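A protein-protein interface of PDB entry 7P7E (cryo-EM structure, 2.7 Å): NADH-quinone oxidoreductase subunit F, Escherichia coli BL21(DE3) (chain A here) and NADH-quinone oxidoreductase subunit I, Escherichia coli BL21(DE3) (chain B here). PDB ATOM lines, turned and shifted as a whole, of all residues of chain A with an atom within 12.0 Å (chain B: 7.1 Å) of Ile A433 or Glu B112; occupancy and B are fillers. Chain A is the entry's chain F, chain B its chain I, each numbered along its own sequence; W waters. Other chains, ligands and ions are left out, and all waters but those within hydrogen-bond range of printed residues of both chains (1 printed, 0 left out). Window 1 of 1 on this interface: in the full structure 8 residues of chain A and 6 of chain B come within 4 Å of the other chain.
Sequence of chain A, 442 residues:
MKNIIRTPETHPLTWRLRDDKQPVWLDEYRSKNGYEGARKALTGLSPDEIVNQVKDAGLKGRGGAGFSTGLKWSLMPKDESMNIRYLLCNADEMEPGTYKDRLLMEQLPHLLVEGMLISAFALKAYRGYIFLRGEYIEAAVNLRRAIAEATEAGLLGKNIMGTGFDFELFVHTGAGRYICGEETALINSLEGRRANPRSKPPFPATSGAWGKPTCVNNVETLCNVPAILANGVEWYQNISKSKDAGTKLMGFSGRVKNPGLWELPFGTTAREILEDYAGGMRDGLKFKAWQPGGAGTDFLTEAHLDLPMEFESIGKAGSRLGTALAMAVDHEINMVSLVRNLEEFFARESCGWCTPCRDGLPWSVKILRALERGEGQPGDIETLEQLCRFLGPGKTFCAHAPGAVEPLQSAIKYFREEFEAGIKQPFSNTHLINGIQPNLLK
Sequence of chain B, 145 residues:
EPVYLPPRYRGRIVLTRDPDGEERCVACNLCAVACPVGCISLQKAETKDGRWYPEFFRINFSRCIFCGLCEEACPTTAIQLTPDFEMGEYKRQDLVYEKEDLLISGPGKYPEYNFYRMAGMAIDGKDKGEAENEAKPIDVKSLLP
N of Asn A434 is in hydrogen-bond range of OE2 of Glu B112 (2.5 Å).
NH2 of Arg B24 sits at hydrogen-bond distance from O of Tyr B110 (2.5 Å).
Glu B112 touches Leu A432 (OE2 to O, 3.6 Å).
Glu B112 touches Ile A433 (OE2 to CA, 3.4 Å).
CD1 of Tyr B110 touches O of Asn A434, 3.8 Å away.
Pro B111 touches Asn A434 (CG to ND2, 3.2 Å).
Gly A435 touches Tyr B110 (O to CE1, 3.5 Å).
Tyr B110 touches Ile A436.
Of the printed residues of chain B, Leu A432 touches Glu B112.
Ile A433 touches just one residue of chain B: Glu B112 (3.4 Å).
Of the printed residues of chain B, Asn A434 touches Tyr B110 (3.8 Å), Pro B111 (3.2 Å) and Glu B112 (2.5 Å).
Of the printed residues of chain B, Gly A435 touches Tyr B110 (3.5 Å).
Of the printed residues of chain B, Ile A436 touches Tyr B110.
No residue of chain A comes within 4 Å of Pro B107.
Of the printed residues of chain A, Tyr B110 touches Asn A434 (3.8 Å), Gly A435 (3.5 Å) and Ile A436 (3.6 Å).
Printed residues of chain A within 4 Å of Pro B111: Asn A434 (3.2 Å).
Glu B112 touches just these residues of chain A: Leu A432 (3.6 Å), Ile A433 (3.4 Å) and Asn A434 (2.5 Å).
Phe B115 touches none of the printed residues of chain A.
Arg B117 touches none of the printed residues of chain A.
The nearest residue of chain B that does not touch Ile A433 is Tyr B113 (4.2 Å).
The nearest residue of chain A that does not touch Glu B112 is Gly A435 (5.7 Å).
Printed residues of chain A that touch a printed residue of chain B: Leu A432, Ile A433, Asn A434, Gly A435 and Ile A436.
Hydrophobic or aromatic side chains of chain A that line the printed part of chain B: Ile A436.
Of the 14 printed residues of chain B, 3 touch a printed residue of chain A.
Printed residues of chain B that touch a printed residue of chain A: Tyr B110, Pro B111 and Glu B112.
Hydrophobic or aromatic side chains of chain B within 4 Å of the printed part of chain A: Tyr B110 and Pro B111.
Among the printed residues, 7 pairs touch across the chains.
Among the printed residues, no Asp or Glu carboxylate lies within 4 Å of a Lys or Arg side-chain nitrogen of the other chain.
Water W1 lies within hydrogen-bond range of the backbone carbonyl oxygen of Asn A434, the backbone NH of Glu B112 and the backbone NH of Tyr B113.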
ATOM      1  N   SER A 428      14.677  12.088 -11.285  1.00  0.00           N
ATOM      2  CA  SER A 428      15.357  12.990 -10.368  1.00  0.00           C
ATOM      3  C   SER A 428      15.518  12.306  -9.021  1.00  0.00           C
ATOM      4  O   SER A 428      14.549  11.767  -8.479  1.00  0.00           O
ATOM      5  CB  SER A 428      14.583  14.302 -10.202  1.00  0.00           C
ATOM      6  OG  SER A 428      15.188  15.130  -9.225  1.00  0.00           O
ATOM      7  N   ASN A 429      16.742  12.325  -8.487  1.00  0.00           N
ATOM      8  CA  ASN A 429      16.962  11.952  -7.095  1.00  0.00           C
ATOM      9  C   ASN A 429      17.932  12.910  -6.412  1.00  0.00           C
ATOM     10  O   ASN A 429      18.484  12.572  -5.358  1.00  0.00           O
ATOM     11  CB  ASN A 429      17.461  10.505  -6.969  1.00  0.00           C
ATOM     12  CG  ASN A 429      18.848  10.301  -7.548  1.00  0.00           C
ATOM     13  OD1 ASN A 429      19.290  11.040  -8.426  1.00  0.00           O
ATOM     14  ND2 ASN A 429      19.541   9.284  -7.055  1.00  0.00           N
ATOM     15  N   THR A 430      18.153  14.089  -6.985  1.00  0.00           N
ATOM     16  CA  THR A 430      19.051  15.093  -6.436  1.00  0.00           C
ATOM     17  C   THR A 430      18.289  16.389  -6.211  1.00  0.00           C
ATOM     18  O   THR A 430      17.613  16.880  -7.121  1.00  0.00           O
ATOM     19  CB  THR A 430      20.235  15.355  -7.372  1.00  0.00           C
ATOM     20  OG1 THR A 430      19.780  15.359  -8.730  1.00  0.00           O
ATOM     21  CG2 THR A 430      21.298  14.294  -7.206  1.00  0.00           C
ATOM     22  N   HIS A 431      18.397  16.937  -5.008  1.00  0.00           N
ATOM     23  CA  HIS A 431      17.938  18.293  -4.771  1.00  0.00           C
ATOM     24  C   HIS A 431      18.973  19.288  -5.285  1.00  0.00           C
ATOM     25  O   HIS A 431      20.154  18.970  -5.446  1.00  0.00           O
ATOM     26  CB  HIS A 431      17.678  18.530  -3.285  1.00  0.00           C
ATOM     27  CG  HIS A 431      16.648  17.617  -2.700  1.00  0.00           C
ATOM     28  ND1 HIS A 431      16.795  17.022  -1.466  1.00  0.00           N
ATOM     29  CD2 HIS A 431      15.453  17.198  -3.180  1.00  0.00           C
ATOM     30  CE1 HIS A 431      15.736  16.274  -1.212  1.00  0.00           C
ATOM     31  NE2 HIS A 431      14.907  16.364  -2.236  1.00  0.00           N
ATOM     32  N   LEU A 432      18.515  20.505  -5.545  1.00  0.00           N
ATOM     33  CA  LEU A 432      19.413  21.573  -5.960  1.00  0.00           C
ATOM     34  C   LEU A 432      20.038  22.207  -4.726  1.00  0.00           C
ATOM     35  O   LEU A 432      19.332  22.793  -3.897  1.00  0.00           O
ATOM     36  CB  LEU A 432      18.666  22.615  -6.786  1.00  0.00           C
ATOM     37  CG  LEU A 432      19.356  23.065  -8.073  1.00  0.00           C
ATOM     38  CD1 LEU A 432      19.612  21.876  -8.983  1.00  0.00           C
ATOM     39  CD2 LEU A 432      18.524  24.117  -8.784  1.00  0.00           C
ATOM     40  N   ILE A 433      21.353  22.084  -4.596  1.00  0.00           N
ATOM     41  CA  ILE A 433      22.093  22.663  -3.481  1.00  0.00           C
ATOM     42  C   ILE A 433      22.612  24.021  -3.922  1.00  0.00           C
ATOM     43  O   ILE A 433      23.360  24.119  -4.902  1.00  0.00           O
ATOM     44  CB  ILE A 433      23.238  21.746  -3.030  1.00  0.00           C
ATOM     45  CG1 ILE A 433      22.678  20.450  -2.445  1.00  0.00           C
ATOM     46  CG2 ILE A 433      24.114  22.449  -2.013  1.00  0.00           C
ATOM     47  CD1 ILE A 433      23.718  19.395  -2.206  1.00  0.00           C
ATOM     48  N   ASN A 434      22.211  25.068  -3.206  1.00  0.00           N
ATOM     49  CA  ASN A 434      22.589  26.423  -3.579  1.00  0.00           C
ATOM     50  C   ASN A 434      24.071  26.652  -3.314  1.00  0.00           C
ATOM     51  O   ASN A 434      24.577  26.341  -2.232  1.00  0.00           O
ATOM     52  CB  ASN A 434      21.746  27.436  -2.806  1.00  0.00           C
ATOM     53  CG  ASN A 434      21.809  28.822  -3.408  1.00  0.00           C
ATOM     54  OD1 ASN A 434      21.989  28.981  -4.614  1.00  0.00           O
ATOM     55  ND2 ASN A 434      21.661  29.837  -2.566  1.00  0.00           N
ATOM     56  N   GLY A 435      24.765  27.199  -4.308  1.00  0.00           N
ATOM     57  CA  GLY A 435      26.192  27.410  -4.233  1.00  0.00           C
ATOM     58  C   GLY A 435      27.025  26.350  -4.921  1.00  0.00           C
ATOM     59  O   GLY A 435      28.242  26.529  -5.046  1.00  0.00           O
ATOM     60  N   ILE A 436      26.413  25.258  -5.368  1.00  0.00           N
ATOM     61  CA  ILE A 436      27.115  24.171  -6.039  1.00  0.00           C
ATOM     62  C   ILE A 436      26.481  23.974  -7.407  1.00  0.00           C
ATOM     63  O   ILE A 436      25.278  23.701  -7.506  1.00  0.00           O
ATOM     64  CB  ILE A 436      27.069  22.872  -5.222  1.00  0.00           C
ATOM     65  CG1 ILE A 436      27.953  22.995  -3.985  1.00  0.00           C
ATOM     66  CG2 ILE A 436      27.512  21.687  -6.066  1.00  0.00           C
ATOM     67  CD1 ILE A 436      27.761  21.887  -2.995  1.00  0.00           C
ATOM     68  N   GLN A 437      27.279  24.120  -8.452  1.00  0.00           N
ATOM     69  CA  GLN A 437      26.797  23.847  -9.800  1.00  0.00           C
ATOM     70  C   GLN A 437      26.801  22.344 -10.050  1.00  0.00           C
ATOM     71  O   GLN A 437      27.817  21.686  -9.811  1.00  0.00           O
ATOM     72  CB  GLN A 437      27.658  24.558 -10.836  1.00  0.00           C
ATOM     73  CG  GLN A 437      27.542  26.071 -10.795  1.00  0.00           C
ATOM     74  CD  GLN A 437      28.534  26.756 -11.711  1.00  0.00           C
ATOM     75  OE1 GLN A 437      29.737  26.745 -11.461  1.00  0.00           O
ATOM     76  NE2 GLN A 437      28.032  27.357 -12.782  1.00  0.00           N
ATOM     77  N   PRO A 438      25.693  21.769 -10.510  1.00  0.00           N
ATOM     78  CA  PRO A 438      25.643  20.318 -10.715  1.00  0.00           C
ATOM     79  C   PRO A 438      26.467  19.879 -11.916  1.00  0.00           C
ATOM     80  O   PRO A 438      26.798  20.661 -12.809  1.00  0.00           O
ATOM     81  CB  PRO A 438      24.153  20.045 -10.939  1.00  0.00           C
ATOM     82  CG  PRO A 438      23.621  21.326 -11.476  1.00  0.00           C
ATOM     83  CD  PRO A 438      24.403  22.415 -10.804  1.00  0.00           C
ATOM     84  N   ASN A 439      26.804  18.590 -11.915  1.00  0.00           N
ATOM     85  CA  ASN A 439      27.510  17.954 -13.026  1.00  0.00           C
ATOM     86  C   ASN A 439      26.461  17.388 -13.973  1.00  0.00           C
ATOM     87  O   ASN A 439      25.963  16.276 -13.793  1.00  0.00           O
ATOM     88  CB  ASN A 439      28.455  16.875 -12.514  1.00  0.00           C
ATOM     89  CG  ASN A 439      29.472  16.449 -13.551  1.00  0.00           C
ATOM     90  OD1 ASN A 439      30.124  17.282 -14.174  1.00  0.00           O
ATOM     91  ND2 ASN A 439      29.611  15.145 -13.742  1.00  0.00           N
ATOM     92  N   LEU A 440      26.124  18.164 -14.999  1.00  0.00           N
ATOM     93  CA  LEU A 440      25.031  17.826 -15.911  1.00  0.00           C
ATOM     94  C   LEU A 440      25.496  16.735 -16.864  1.00  0.00           C
ATOM     95  O   LEU A 440      26.076  17.002 -17.917  1.00  0.00           O
ATOM     96  CB  LEU A 440      24.567  19.065 -16.665  1.00  0.00           C
ATOM     97  CG  LEU A 440      24.072  20.212 -15.782  1.00  0.00           C
ATOM     98  CD1 LEU A 440      23.881  21.479 -16.600  1.00  0.00           C
ATOM     99  CD2 LEU A 440      22.784  19.819 -15.079  1.00  0.00           C
ATOM    100  N   ASP B  18      25.544  26.057  10.255  1.00  0.00           N
ATOM    101  CA  ASP B  18      24.323  25.649   9.590  1.00  0.00           C
ATOM    102  C   ASP B  18      23.242  26.726   9.741  1.00  0.00           C
ATOM    103  O   ASP B  18      23.377  27.633  10.565  1.00  0.00           O
ATOM    104  CB  ASP B  18      23.909  24.251  10.094  1.00  0.00           C
ATOM    105  CG  ASP B  18      23.347  24.216  11.533  1.00  0.00           C
ATOM    106  OD1 ASP B  18      23.028  25.236  12.177  1.00  0.00           O
ATOM    107  OD2 ASP B  18      23.283  23.090  12.067  1.00  0.00           O
ATOM    108  N   PRO B  19      22.186  26.678   8.915  1.00  0.00           N
ATOM    109  CA  PRO B  19      21.087  27.651   9.080  1.00  0.00           C
ATOM    110  C   PRO B  19      20.411  27.611  10.441  1.00  0.00           C
ATOM    111  O   PRO B  19      19.834  28.621  10.861  1.00  0.00           O
ATOM    112  CB  PRO B  19      20.115  27.262   7.961  1.00  0.00           C
ATOM    113  CG  PRO B  19      20.972  26.688   6.912  1.00  0.00           C
ATOM    114  CD  PRO B  19      22.117  26.004   7.605  1.00  0.00           C
ATOM    115  N   ARG B  24      28.841  23.765  11.449  1.00  0.00           N
ATOM    116  CA  ARG B  24      28.670  22.711  10.461  1.00  0.00           C
ATOM    117  C   ARG B  24      29.675  21.582  10.621  1.00  0.00           C
ATOM    118  O   ARG B  24      29.403  20.466  10.167  1.00  0.00           O
ATOM    119  CB  ARG B  24      28.788  23.287   9.055  1.00  0.00           C
ATOM    120  CG  ARG B  24      27.495  23.757   8.455  1.00  0.00           C
ATOM    121  CD  ARG B  24      27.761  24.404   7.121  1.00  0.00           C
ATOM    122  NE  ARG B  24      26.537  24.648   6.373  1.00  0.00           N
ATOM    123  CZ  ARG B  24      26.399  25.608   5.473  1.00  0.00           C
ATOM    124  NH1 ARG B  24      27.392  26.430   5.184  1.00  0.00           N
ATOM    125  NH2 ARG B  24      25.236  25.746   4.845  1.00  0.00           N
ATOM    126  N   THR B  77      30.358  21.165   4.008  1.00  0.00           N
ATOM    127  CA  THR B  77      30.596  22.564   3.618  1.00  0.00           C
ATOM    128  C   THR B  77      30.903  23.448   4.824  1.00  0.00           C
ATOM    129  O   THR B  77      30.525  24.618   4.863  1.00  0.00           O
ATOM    130  CB  THR B  77      29.433  23.149   2.807  1.00  0.00           C
ATOM    131  OG1 THR B  77      28.299  23.357   3.657  1.00  0.00           O
ATOM    132  CG2 THR B  77      29.048  22.224   1.670  1.00  0.00           C
ATOM    133  N   PRO B 107      26.416  31.015   7.326  1.00  0.00           N
ATOM    134  CA  PRO B 107      26.663  29.856   6.457  1.00  0.00           C
ATOM    135  C   PRO B 107      27.711  30.074   5.382  1.00  0.00           C
ATOM    136  O   PRO B 107      28.112  29.096   4.737  1.00  0.00           O
ATOM    137  CB  PRO B 107      25.289  29.603   5.832  1.00  0.00           C
ATOM    138  CG  PRO B 107      24.669  30.944   5.779  1.00  0.00           C
ATOM    139  CD  PRO B 107      25.143  31.681   7.001  1.00  0.00           C
ATOM    140  N   LYS B 109      29.391  30.698   1.893  1.00  0.00           N
ATOM    141  CA  LYS B 109      29.049  30.590   0.480  1.00  0.00           C
ATOM    142  C   LYS B 109      27.931  29.594   0.204  1.00  0.00           C
ATOM    143  O   LYS B 109      27.355  29.623  -0.888  1.00  0.00           O
ATOM    144  CB  LYS B 109      30.288  30.201  -0.327  1.00  0.00           C
ATOM    145  CG  LYS B 109      31.437  31.183  -0.202  1.00  0.00           C
ATOM    146  CD  LYS B 109      32.576  30.827  -1.140  1.00  0.00           C
ATOM    147  CE  LYS B 109      33.375  29.652  -0.613  1.00  0.00           C
ATOM    148  NZ  LYS B 109      34.541  29.343  -1.485  1.00  0.00           N
ATOM    149  N   TYR B 110      27.617  28.714   1.149  1.00  0.00           N
ATOM    150  CA  TYR B 110      26.554  27.721   0.980  1.00  0.00           C
ATOM    151  C   TYR B 110      25.467  27.997   2.005  1.00  0.00           C
ATOM    152  O   TYR B 110      25.602  27.609   3.178  1.00  0.00           O
ATOM    153  CB  TYR B 110      27.106  26.305   1.128  1.00  0.00           C
ATOM    154  CG  TYR B 110      28.325  26.057   0.271  1.00  0.00           C
ATOM    155  CD1 TYR B 110      28.197  25.759  -1.077  1.00  0.00           C
ATOM    156  CD2 TYR B 110      29.602  26.142   0.805  1.00  0.00           C
ATOM    157  CE1 TYR B 110      29.308  25.541  -1.865  1.00  0.00           C
ATOM    158  CE2 TYR B 110      30.718  25.925   0.026  1.00  0.00           C
ATOM    159  CZ  TYR B 110      30.564  25.625  -1.308  1.00  0.00           C
ATOM    160  OH  TYR B 110      31.675  25.408  -2.090  1.00  0.00           O
ATOM    161  N   PRO B 111      24.372  28.655   1.616  1.00  0.00           N
ATOM    162  CA  PRO B 111      23.463  29.223   2.622  1.00  0.00           C
ATOM    163  C   PRO B 111      22.492  28.242   3.255  1.00  0.00           C
ATOM    164  O   PRO B 111      21.964  28.552   4.330  1.00  0.00           O
ATOM    165  CB  PRO B 111      22.705  30.296   1.833  1.00  0.00           C
ATOM    166  CG  PRO B 111      22.709  29.795   0.442  1.00  0.00           C
ATOM    167  CD  PRO B 111      23.998  29.047   0.248  1.00  0.00           C
ATOM    168  N   GLU B 112      22.226  27.085   2.652  1.00  0.00           N
ATOM    169  CA  GLU B 112      21.139  26.242   3.124  1.00  0.00           C
ATOM    170  C   GLU B 112      21.524  24.811   3.467  1.00  0.00           C
ATOM    171  O   GLU B 112      20.697  24.103   4.050  1.00  0.00           O
ATOM    172  CB  GLU B 112      20.002  26.203   2.088  1.00  0.00           C
ATOM    173  CG  GLU B 112      20.464  26.192   0.639  1.00  0.00           C
ATOM    174  CD  GLU B 112      20.497  24.799   0.034  1.00  0.00           C
ATOM    175  OE1 GLU B 112      20.295  23.812   0.772  1.00  0.00           O
ATOM    176  OE2 GLU B 112      20.726  24.692  -1.189  1.00  0.00           O
ATOM    177  N   TYR B 113      22.729  24.359   3.129  1.00  0.00           N
ATOM    178  CA  TYR B 113      23.053  22.949   3.308  1.00  0.00           C
ATOM    179  C   TYR B 113      23.248  22.610   4.779  1.00  0.00           C
ATOM    180  O   TYR B 113      23.932  23.329   5.512  1.00  0.00           O
ATOM    181  CB  TYR B 113      24.302  22.565   2.521  1.00  0.00           C
ATOM    182  CG  TYR B 113      24.606  21.089   2.626  1.00  0.00           C
ATOM    183  CD1 TYR B 113      23.853  20.158   1.923  1.00  0.00           C
ATOM    184  CD2 TYR B 113      25.624  20.623   3.447  1.00  0.00           C
ATOM    185  CE1 TYR B 113      24.114  18.809   2.023  1.00  0.00           C
ATOM    186  CE2 TYR B 113      25.891  19.275   3.554  1.00  0.00           C
ATOM    187  CZ  TYR B 113      25.134  18.372   2.838  1.00  0.00           C
ATOM    188  OH  TYR B 113      25.396  17.030   2.939  1.00  0.00           O
ATOM    189  N   ASN B 114      22.644  21.504   5.201  1.00  0.00           N
ATOM    190  CA  ASN B 114      22.794  20.973   6.548  1.00  0.00           C
ATOM    191  C   ASN B 114      23.111  19.492   6.422  1.00  0.00           C
ATOM    192  O   ASN B 114      22.279  18.723   5.933  1.00  0.00           O
ATOM    193  CB  ASN B 114      21.522  21.191   7.371  1.00  0.00           C
ATOM    194  CG  ASN B 114      21.758  21.066   8.861  1.00  0.00           C
ATOM    195  OD1 ASN B 114      22.793  20.572   9.302  1.00  0.00           O
ATOM    196  ND2 ASN B 114      20.792  21.516   9.648  1.00  0.00           N
ATOM    197  N   PHE B 115      24.317  19.101   6.842  1.00  0.00           N
ATOM    198  CA  PHE B 115      24.705  17.696   6.768  1.00  0.00           C
ATOM    199  C   PHE B 115      23.849  16.841   7.686  1.00  0.00           C
ATOM    200  O   PHE B 115      23.478  15.717   7.331  1.00  0.00           O
ATOM    201  CB  PHE B 115      26.184  17.530   7.118  1.00  0.00           C
ATOM    202  CG  PHE B 115      26.582  16.107   7.402  1.00  0.00           C
ATOM    203  CD1 PHE B 115      26.753  15.206   6.366  1.00  0.00           C
ATOM    204  CD2 PHE B 115      26.783  15.670   8.702  1.00  0.00           C
ATOM    205  CE1 PHE B 115      27.112  13.898   6.620  1.00  0.00           C
ATOM    206  CE2 PHE B 115      27.139  14.363   8.960  1.00  0.00           C
ATOM    207  CZ  PHE B 115      27.307  13.479   7.919  1.00  0.00           C
ATOM    208  N   ARG B 117      20.829  17.101   8.443  1.00  0.00           N
ATOM    209  CA  ARG B 117      19.539  16.769   7.859  1.00  0.00           C
ATOM    210  C   ARG B 117      19.614  15.563   6.933  1.00  0.00           C
ATOM    211  O   ARG B 117      18.569  15.017   6.569  1.00  0.00           O
ATOM    212  CB  ARG B 117      18.979  17.970   7.095  1.00  0.00           C
ATOM    213  CG  ARG B 117      18.460  19.083   7.986  1.00  0.00           C
ATOM    214  CD  ARG B 117      17.026  18.829   8.406  1.00  0.00           C
ATOM    215  NE  ARG B 117      16.302  18.036   7.420  1.00  0.00           N
ATOM    216  CZ  ARG B 117      15.569  16.968   7.707  1.00  0.00           C
ATOM    217  NH1 ARG B 117      15.435  16.536   8.950  1.00  0.00           N
ATOM    218  NH2 ARG B 117      14.955  16.319   6.722  1.00  0.00           N
ATOM    219  N   MET B 118      20.817  15.137   6.548  1.00  0.00           N
ATOM    220  CA  MET B 118      21.019  13.975   5.692  1.00  0.00           C
ATOM    221  C   MET B 118      21.428  12.730   6.464  1.00  0.00           C
ATOM    222  O   MET B 118      21.035  11.622   6.091  1.00  0.00           O
ATOM    223  CB  MET B 118      22.095  14.266   4.640  1.00  0.00           C
ATOM    224  CG  MET B 118      21.935  15.567   3.882  1.00  0.00           C
ATOM    225  SD  MET B 118      20.625  15.518   2.653  1.00  0.00           S
ATOM    226  CE  MET B 118      20.181  17.248   2.595  1.00  0.00           C
HETATM  227  O   HOH W   1      23.673  25.473   0.192  1.00  0.00           O
